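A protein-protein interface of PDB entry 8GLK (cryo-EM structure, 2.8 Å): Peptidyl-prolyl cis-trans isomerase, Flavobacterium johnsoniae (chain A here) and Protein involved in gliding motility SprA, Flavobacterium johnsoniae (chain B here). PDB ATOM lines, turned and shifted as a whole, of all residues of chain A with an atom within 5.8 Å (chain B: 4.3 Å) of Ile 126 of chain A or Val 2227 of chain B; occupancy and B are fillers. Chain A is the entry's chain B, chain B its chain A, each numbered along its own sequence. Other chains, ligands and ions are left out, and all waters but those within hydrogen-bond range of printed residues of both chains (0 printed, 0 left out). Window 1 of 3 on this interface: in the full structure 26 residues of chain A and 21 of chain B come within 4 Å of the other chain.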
ATOM      1  N   THR A 124      -1.528  12.450  -4.257  1.00  0.00           N
ATOM      2  CA  THR A 124      -0.769  13.207  -5.240  1.00  0.00           C
ATOM      3  C   THR A 124       0.538  13.751  -4.682  1.00  0.00           C
ATOM      4  O   THR A 124       1.275  14.423  -5.409  1.00  0.00           O
ATOM      5  CB  THR A 124      -1.621  14.360  -5.778  1.00  0.00           C
ATOM      6  OG1 THR A 124      -1.813  15.336  -4.747  1.00  0.00           O
ATOM      7  CG2 THR A 124      -2.976  13.848  -6.238  1.00  0.00           C
ATOM      8  N   LEU A 125       0.841  13.475  -3.417  1.00  0.00           N
ATOM      9  CA  LEU A 125       2.003  14.038  -2.753  1.00  0.00           C
ATOM     10  C   LEU A 125       3.208  13.112  -2.898  1.00  0.00           C
ATOM     11  O   LEU A 125       3.132  12.034  -3.492  1.00  0.00           O
ATOM     12  CB  LEU A 125       1.689  14.305  -1.282  1.00  0.00           C
ATOM     13  CG  LEU A 125       0.372  15.035  -1.019  1.00  0.00           C
ATOM     14  CD1 LEU A 125       0.101  15.142   0.468  1.00  0.00           C
ATOM     15  CD2 LEU A 125       0.390  16.410  -1.660  1.00  0.00           C
ATOM     16  N   ILE A 126       4.339  13.544  -2.351  1.00  0.00           N
ATOM     17  CA  ILE A 126       5.576  12.768  -2.387  1.00  0.00           C
ATOM     18  C   ILE A 126       5.405  11.533  -1.509  1.00  0.00           C
ATOM     19  O   ILE A 126       4.579  11.545  -0.585  1.00  0.00           O
ATOM     20  CB  ILE A 126       6.777  13.616  -1.938  1.00  0.00           C
ATOM     21  CG1 ILE A 126       6.499  14.260  -0.579  1.00  0.00           C
ATOM     22  CG2 ILE A 126       7.095  14.678  -2.977  1.00  0.00           C
ATOM     23  CD1 ILE A 126       7.604  15.174  -0.097  1.00  0.00           C
ATOM     24  N   PRO A 127       6.144  10.448  -1.765  1.00  0.00           N
ATOM     25  CA  PRO A 127       5.983   9.243  -0.933  1.00  0.00           C
ATOM     26  C   PRO A 127       6.247   9.473   0.544  1.00  0.00           C
ATOM     27  O   PRO A 127       5.606   8.824   1.382  1.00  0.00           O
ATOM     28  CB  PRO A 127       7.003   8.267  -1.540  1.00  0.00           C
ATOM     29  CG  PRO A 127       7.157   8.719  -2.948  1.00  0.00           C
ATOM     30  CD  PRO A 127       7.027  10.212  -2.920  1.00  0.00           C
ATOM     31  N   GLY A 128       7.165  10.378   0.890  1.00  0.00           N
ATOM     32  CA  GLY A 128       7.439  10.639   2.295  1.00  0.00           C
ATOM     33  C   GLY A 128       6.209  11.101   3.052  1.00  0.00           C
ATOM     34  O   GLY A 128       5.953  10.658   4.174  1.00  0.00           O
ATOM     35  N   TRP A 129       5.425  11.992   2.444  1.00  0.00           N
ATOM     36  CA  TRP A 129       4.159  12.383   3.052  1.00  0.00           C
ATOM     37  C   TRP A 129       3.205  11.200   3.130  1.00  0.00           C
ATOM     38  O   TRP A 129       2.510  11.020   4.137  1.00  0.00           O
ATOM     39  CB  TRP A 129       3.526  13.528   2.263  1.00  0.00           C
ATOM     40  CG  TRP A 129       4.082  14.870   2.599  1.00  0.00           C
ATOM     41  CD1 TRP A 129       5.398  15.228   2.628  1.00  0.00           C
ATOM     42  CD2 TRP A 129       3.341  16.039   2.957  1.00  0.00           C
ATOM     43  NE1 TRP A 129       5.521  16.550   2.977  1.00  0.00           N
ATOM     44  CE2 TRP A 129       4.271  17.070   3.185  1.00  0.00           C
ATOM     45  CE3 TRP A 129       1.980  16.314   3.108  1.00  0.00           C
ATOM     46  CZ2 TRP A 129       3.883  18.353   3.554  1.00  0.00           C
ATOM     47  CZ3 TRP A 129       1.597  17.585   3.471  1.00  0.00           C
ATOM     48  CH2 TRP A 129       2.543  18.589   3.692  1.00  0.00           C
ATOM     49  N   LYS A 130       3.169  10.374   2.079  1.00  0.00           N
ATOM     50  CA  LYS A 130       2.285   9.211   2.070  1.00  0.00           C
ATOM     51  C   LYS A 130       2.601   8.249   3.207  1.00  0.00           C
ATOM     52  O   LYS A 130       1.711   7.527   3.669  1.00  0.00           O
ATOM     53  CB  LYS A 130       2.382   8.485   0.730  1.00  0.00           C
ATOM     54  CG  LYS A 130       1.846   9.267  -0.449  1.00  0.00           C
ATOM     55  CD  LYS A 130       1.953   8.450  -1.722  1.00  0.00           C
ATOM     56  CE  LYS A 130       1.396   9.206  -2.910  1.00  0.00           C
ATOM     57  NZ  LYS A 130       1.479   8.406  -4.161  1.00  0.00           N
ATOM     58  N   GLU A 131       3.854   8.208   3.660  1.00  0.00           N
ATOM     59  CA  GLU A 131       4.203   7.356   4.790  1.00  0.00           C
ATOM     60  C   GLU A 131       4.173   8.080   6.130  1.00  0.00           C
ATOM     61  O   GLU A 131       4.115   7.416   7.170  1.00  0.00           O
ATOM     62  CB  GLU A 131       5.588   6.731   4.593  1.00  0.00           C
ATOM     63  CG  GLU A 131       5.903   6.345   3.162  1.00  0.00           C
ATOM     64  CD  GLU A 131       6.956   5.263   3.073  1.00  0.00           C
ATOM     65  OE1 GLU A 131       7.047   4.606   2.015  1.00  0.00           O
ATOM     66  OE2 GLU A 131       7.694   5.072   4.062  1.00  0.00           O
ATOM     67  N   VAL A 146      12.461  13.272   5.040  1.00  0.00           N
ATOM     68  CA  VAL A 146      12.282  12.492   3.810  1.00  0.00           C
ATOM     69  C   VAL A 146      13.585  12.463   3.018  1.00  0.00           C
ATOM     70  O   VAL A 146      14.182  13.529   2.762  1.00  0.00           O
ATOM     71  CB  VAL A 146      11.145  13.089   2.965  1.00  0.00           C
ATOM     72  CG1 VAL A 146      10.972  12.305   1.684  1.00  0.00           C
ATOM     73  CG2 VAL A 146       9.849  13.125   3.760  1.00  0.00           C
ATOM     74  N   LEU A 150      12.420   9.054  -1.580  1.00  0.00           N
ATOM     75  CA  LEU A 150      11.064   9.258  -1.092  1.00  0.00           C
ATOM     76  C   LEU A 150      10.589  10.694  -1.267  1.00  0.00           C
ATOM     77  O   LEU A 150       9.449  11.002  -0.907  1.00  0.00           O
ATOM     78  CB  LEU A 150      10.967   8.861   0.384  1.00  0.00           C
ATOM     79  CG  LEU A 150      11.089   7.370   0.702  1.00  0.00           C
ATOM     80  CD1 LEU A 150      10.814   7.111   2.173  1.00  0.00           C
ATOM     81  CD2 LEU A 150      10.146   6.558  -0.172  1.00  0.00           C
ATOM     82  N   GLY A 151      11.432  11.573  -1.803  1.00  0.00           N
ATOM     83  CA  GLY A 151      11.065  12.962  -1.989  1.00  0.00           C
ATOM     84  C   GLY A 151      10.890  13.339  -3.445  1.00  0.00           C
ATOM     85  O   GLY A 151       9.937  12.900  -4.095  1.00  0.00           O
ATOM     86  N   TYR A 152      11.803  14.154  -3.971  1.00  0.00           N
ATOM     87  CA  TYR A 152      11.745  14.597  -5.356  1.00  0.00           C
ATOM     88  C   TYR A 152      12.694  13.822  -6.263  1.00  0.00           C
ATOM     89  O   TYR A 152      12.886  14.212  -7.418  1.00  0.00           O
ATOM     90  CB  TYR A 152      12.034  16.095  -5.447  1.00  0.00           C
ATOM     91  CG  TYR A 152      10.943  16.955  -4.852  1.00  0.00           C
ATOM     92  CD1 TYR A 152       9.720  17.098  -5.492  1.00  0.00           C
ATOM     93  CD2 TYR A 152      11.138  17.629  -3.657  1.00  0.00           C
ATOM     94  CE1 TYR A 152       8.719  17.883  -4.951  1.00  0.00           C
ATOM     95  CE2 TYR A 152      10.144  18.416  -3.109  1.00  0.00           C
ATOM     96  CZ  TYR A 152       8.936  18.540  -3.761  1.00  0.00           C
ATOM     97  OH  TYR A 152       7.944  19.324  -3.220  1.00  0.00           O
ATOM     98  N   LEU A 166      15.011  16.327   2.736  1.00  0.00           N
ATOM     99  CA  LEU A 166      13.968  17.324   2.937  1.00  0.00           C
ATOM    100  C   LEU A 166      13.419  17.182   4.347  1.00  0.00           C
ATOM    101  O   LEU A 166      12.971  16.097   4.732  1.00  0.00           O
ATOM    102  CB  LEU A 166      12.847  17.137   1.914  1.00  0.00           C
ATOM    103  CG  LEU A 166      13.246  17.230   0.441  1.00  0.00           C
ATOM    104  CD1 LEU A 166      12.054  16.906  -0.437  1.00  0.00           C
ATOM    105  CD2 LEU A 166      13.824  18.587   0.097  1.00  0.00           C
ATOM    106  N   PHE A 168      10.520  18.343   6.879  1.00  0.00           N
ATOM    107  CA  PHE A 168       9.174  18.896   6.865  1.00  0.00           C
ATOM    108  C   PHE A 168       8.637  18.977   8.285  1.00  0.00           C
ATOM    109  O   PHE A 168       8.812  18.045   9.072  1.00  0.00           O
ATOM    110  CB  PHE A 168       8.228  18.033   6.021  1.00  0.00           C
ATOM    111  CG  PHE A 168       8.354  18.255   4.545  1.00  0.00           C
ATOM    112  CD1 PHE A 168       7.716  19.321   3.938  1.00  0.00           C
ATOM    113  CD2 PHE A 168       9.092  17.386   3.760  1.00  0.00           C
ATOM    114  CE1 PHE A 168       7.824  19.527   2.579  1.00  0.00           C
ATOM    115  CE2 PHE A 168       9.202  17.584   2.399  1.00  0.00           C
ATOM    116  CZ  PHE A 168       8.566  18.656   1.808  1.00  0.00           C
ATOM    117  N   PRO B2225       4.526  19.734  -2.253  1.00  0.00           N
ATOM    118  CA  PRO B2225       4.629  18.266  -2.218  1.00  0.00           C
ATOM    119  C   PRO B2225       3.758  17.572  -3.249  1.00  0.00           C
ATOM    120  O   PRO B2225       4.030  16.413  -3.584  1.00  0.00           O
ATOM    121  CB  PRO B2225       4.194  17.915  -0.788  1.00  0.00           C
ATOM    122  CG  PRO B2225       3.403  19.095  -0.327  1.00  0.00           C
ATOM    123  CD  PRO B2225       4.049  20.279  -0.971  1.00  0.00           C
ATOM    124  N   LYS B2226       2.725  18.239  -3.759  1.00  0.00           N
ATOM    125  CA  LYS B2226       1.864  17.659  -4.785  1.00  0.00           C
ATOM    126  C   LYS B2226       2.676  17.433  -6.055  1.00  0.00           C
ATOM    127  O   LYS B2226       3.066  18.390  -6.730  1.00  0.00           O
ATOM    128  CB  LYS B2226       0.675  18.578  -5.048  1.00  0.00           C
ATOM    129  CG  LYS B2226      -0.395  17.981  -5.942  1.00  0.00           C
ATOM    130  CD  LYS B2226      -1.439  19.020  -6.312  1.00  0.00           C
ATOM    131  CE  LYS B2226      -2.607  18.394  -7.053  1.00  0.00           C
ATOM    132  NZ  LYS B2226      -2.169  17.665  -8.273  1.00  0.00           N
ATOM    133  N   VAL B2227       2.930  16.169  -6.383  1.00  0.00           N
ATOM    134  CA  VAL B2227       3.775  15.820  -7.519  1.00  0.00           C
ATOM    135  C   VAL B2227       3.049  15.010  -8.581  1.00  0.00           C
ATOM    136  O   VAL B2227       3.591  14.843  -9.683  1.00  0.00           O
ATOM    137  CB  VAL B2227       5.045  15.066  -7.066  1.00  0.00           C
ATOM    138  CG1 VAL B2227       5.960  15.992  -6.284  1.00  0.00           C
ATOM    139  CG2 VAL B2227       4.671  13.849  -6.235  1.00  0.00           C
ATOM    140  N   GLN B2228       1.850  14.506  -8.303  1.00  0.00           N
ATOM    141  CA  GLN B2228       1.117  13.670  -9.240  1.00  0.00           C
ATOM    142  C   GLN B2228      -0.218  14.313  -9.587  1.00  0.00           C
ATOM    143  O   GLN B2228      -0.836  14.988  -8.760  1.00  0.00           O
ATOM    144  CB  GLN B2228       0.892  12.264  -8.671  1.00  0.00           C
ATOM    145  CG  GLN B2228       2.150  11.413  -8.625  1.00  0.00           C
ATOM    146  CD  GLN B2228       1.946  10.105  -7.887  1.00  0.00           C
ATOM    147  OE1 GLN B2228       0.830   9.769  -7.492  1.00  0.00           O
ATOM    148  NE2 GLN B2228       3.026   9.356  -7.703  1.00  0.00           N
ATOM    149  N   ASN B2233       0.156  10.646 -12.804  1.00  0.00           N
ATOM    150  CA  ASN B2233       1.373  10.954 -13.538  1.00  0.00           C
ATOM    151  C   ASN B2233       2.131  12.079 -12.850  1.00  0.00           C
ATOM    152  O   ASN B2233       1.528  13.023 -12.333  1.00  0.00           O
ATOM    153  CB  ASN B2233       1.048  11.362 -14.977  1.00  0.00           C
ATOM    154  CG  ASN B2233       0.689  10.185 -15.848  1.00  0.00           C
ATOM    155  OD1 ASN B2233       1.327   9.137 -15.787  1.00  0.00           O
ATOM    156  ND2 ASN B2233      -0.339  10.348 -16.670  1.00  0.00           N
ATOM    157  N   PHE B2234       3.457  11.975 -12.847  1.00  0.00           N
ATOM    158  CA  PHE B2234       4.276  13.072 -12.354  1.00  0.00           C
ATOM    159  C   PHE B2234       4.081  14.301 -13.231  1.00  0.00           C
ATOM    160  O   PHE B2234       3.979  14.201 -14.456  1.00  0.00           O
ATOM    161  CB  PHE B2234       5.753  12.680 -12.328  1.00  0.00           C
ATOM    162  CG  PHE B2234       6.126  11.788 -11.182  1.00  0.00           C
ATOM    163  CD1 PHE B2234       5.477  11.896  -9.966  1.00  0.00           C
ATOM    164  CD2 PHE B2234       7.140  10.856 -11.316  1.00  0.00           C
ATOM    165  CE1 PHE B2234       5.822  11.080  -8.908  1.00  0.00           C
ATOM    166  CE2 PHE B2234       7.489  10.038 -10.261  1.00  0.00           C
ATOM    167  CZ  PHE B2234       6.829  10.150  -9.056  1.00  0.00           C
ATOM    168  N   TYR B2235       4.022  15.466 -12.594  1.00  0.00           N
ATOM    169  CA  TYR B2235       3.870  16.708 -13.336  1.00  0.00           C
ATOM    170  C   TYR B2235       5.111  16.977 -14.177  1.00  0.00           C
ATOM    171  O   TYR B2235       6.243  16.779 -13.726  1.00  0.00           O
ATOM    172  CB  TYR B2235       3.616  17.872 -12.380  1.00  0.00           C
ATOM    173  CG  TYR B2235       2.192  17.948 -11.883  1.00  0.00           C
ATOM    174  CD1 TYR B2235       1.135  18.078 -12.771  1.00  0.00           C
ATOM    175  CD2 TYR B2235       1.905  17.888 -10.527  1.00  0.00           C
ATOM    176  CE1 TYR B2235      -0.167  18.149 -12.322  1.00  0.00           C
ATOM    177  CE2 TYR B2235       0.605  17.959 -10.070  1.00  0.00           C
ATOM    178  CZ  TYR B2235      -0.426  18.089 -10.973  1.00  0.00           C
ATOM    179  OH  TYR B2235      -1.724  18.159 -10.524  1.00  0.00           O
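Ile 126 of chain A touches just these residues of chain B: Pro 2225 and Val 2227.
Val 146 of chain A touches none of the printed residues of chain B.
Leu 150 of chain A touches none of the printed residues of chain B.
Printed residues of chain A within 4 Å of Lys 2226 of chain B: Thr 124 (3.2 Å) and Leu 125 (3.6 Å).
Of chain A, only Thr 124, Leu 125, Ile 126 and Tyr 152 come within 4 Å of Val 2227 of chain B.
Of the printed residues of chain A, Gln 2228 of chain B touches Thr 124 and Lys 130.
The nearest printed residue of chain B that does not touch Leu 125 of chain A is Gln 2228 of chain B (4.9 Å).
N of Tyr 2235 of chain B is in hydrogen-bond range of O of Val 2227 of chain B.
The side-chain amino group (NZ) of Lys 2226 of chain B lies within hydrogen-bond range of the backbone carbonyl oxygen (O) of Gln 2228 of chain B, at 3.0 Å.
Hydrophobic or aromatic side chains of chain A that line the printed part of chain B: Leu 125, Ile 126, Trp 129 and Tyr 152.
Hydrophobic or aromatic side chains of chain B that line the printed part of chain A: Pro 2225 and Val 2227.
Among the printed residues, 13 pairs touch across the chains.
Among the printed residues, no Asp or Glu carboxylate lies within 4 Å of a Lys or Arg side-chain nitrogen of the other chain.
Pro 2225 of chain B touches Thr 124 of chain A.
Thr 124 of chain A touches Lys 2226 of chain B.
Pro 2225 of chain B touches Leu 125 of chain A (O to CA, 3.2 Å).
N of Lys 2226 of chain B touches CD2 of Leu 125 of chain A, 3.6 Å away.
O of Leu 125 of chain A touches CG2 of Val 2227 of chain B, at 3.6 Å.
Ile 126 of chain A touches Val 2227 of chain B (CG2 to CG1, 3.7 Å).
CZ2 of Trp 129 of chain A touches CG of Pro 2225 of chain B (3.98 Å).
Gln 2228 of chain B touches Lys 130 of chain A.
Tyr 152 of chain A touches Pro 2225 of chain B.
Val 2227 of chain B touches Tyr 152 of chain A.
The backbone NH of Gln 2228 of chain B is in hydrogen-bond range of the backbone carbonyl oxygen of Thr 124 of chain A (3.0 Å).
The backbone carbonyl oxygen of Thr 124 of chain A lies within hydrogen-bond range of the backbone NH of Val 2227 of chain B (2.6 Å).
O of Pro 2225 of chain B sits at hydrogen-bond distance from N of Ile 126 of chain A.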
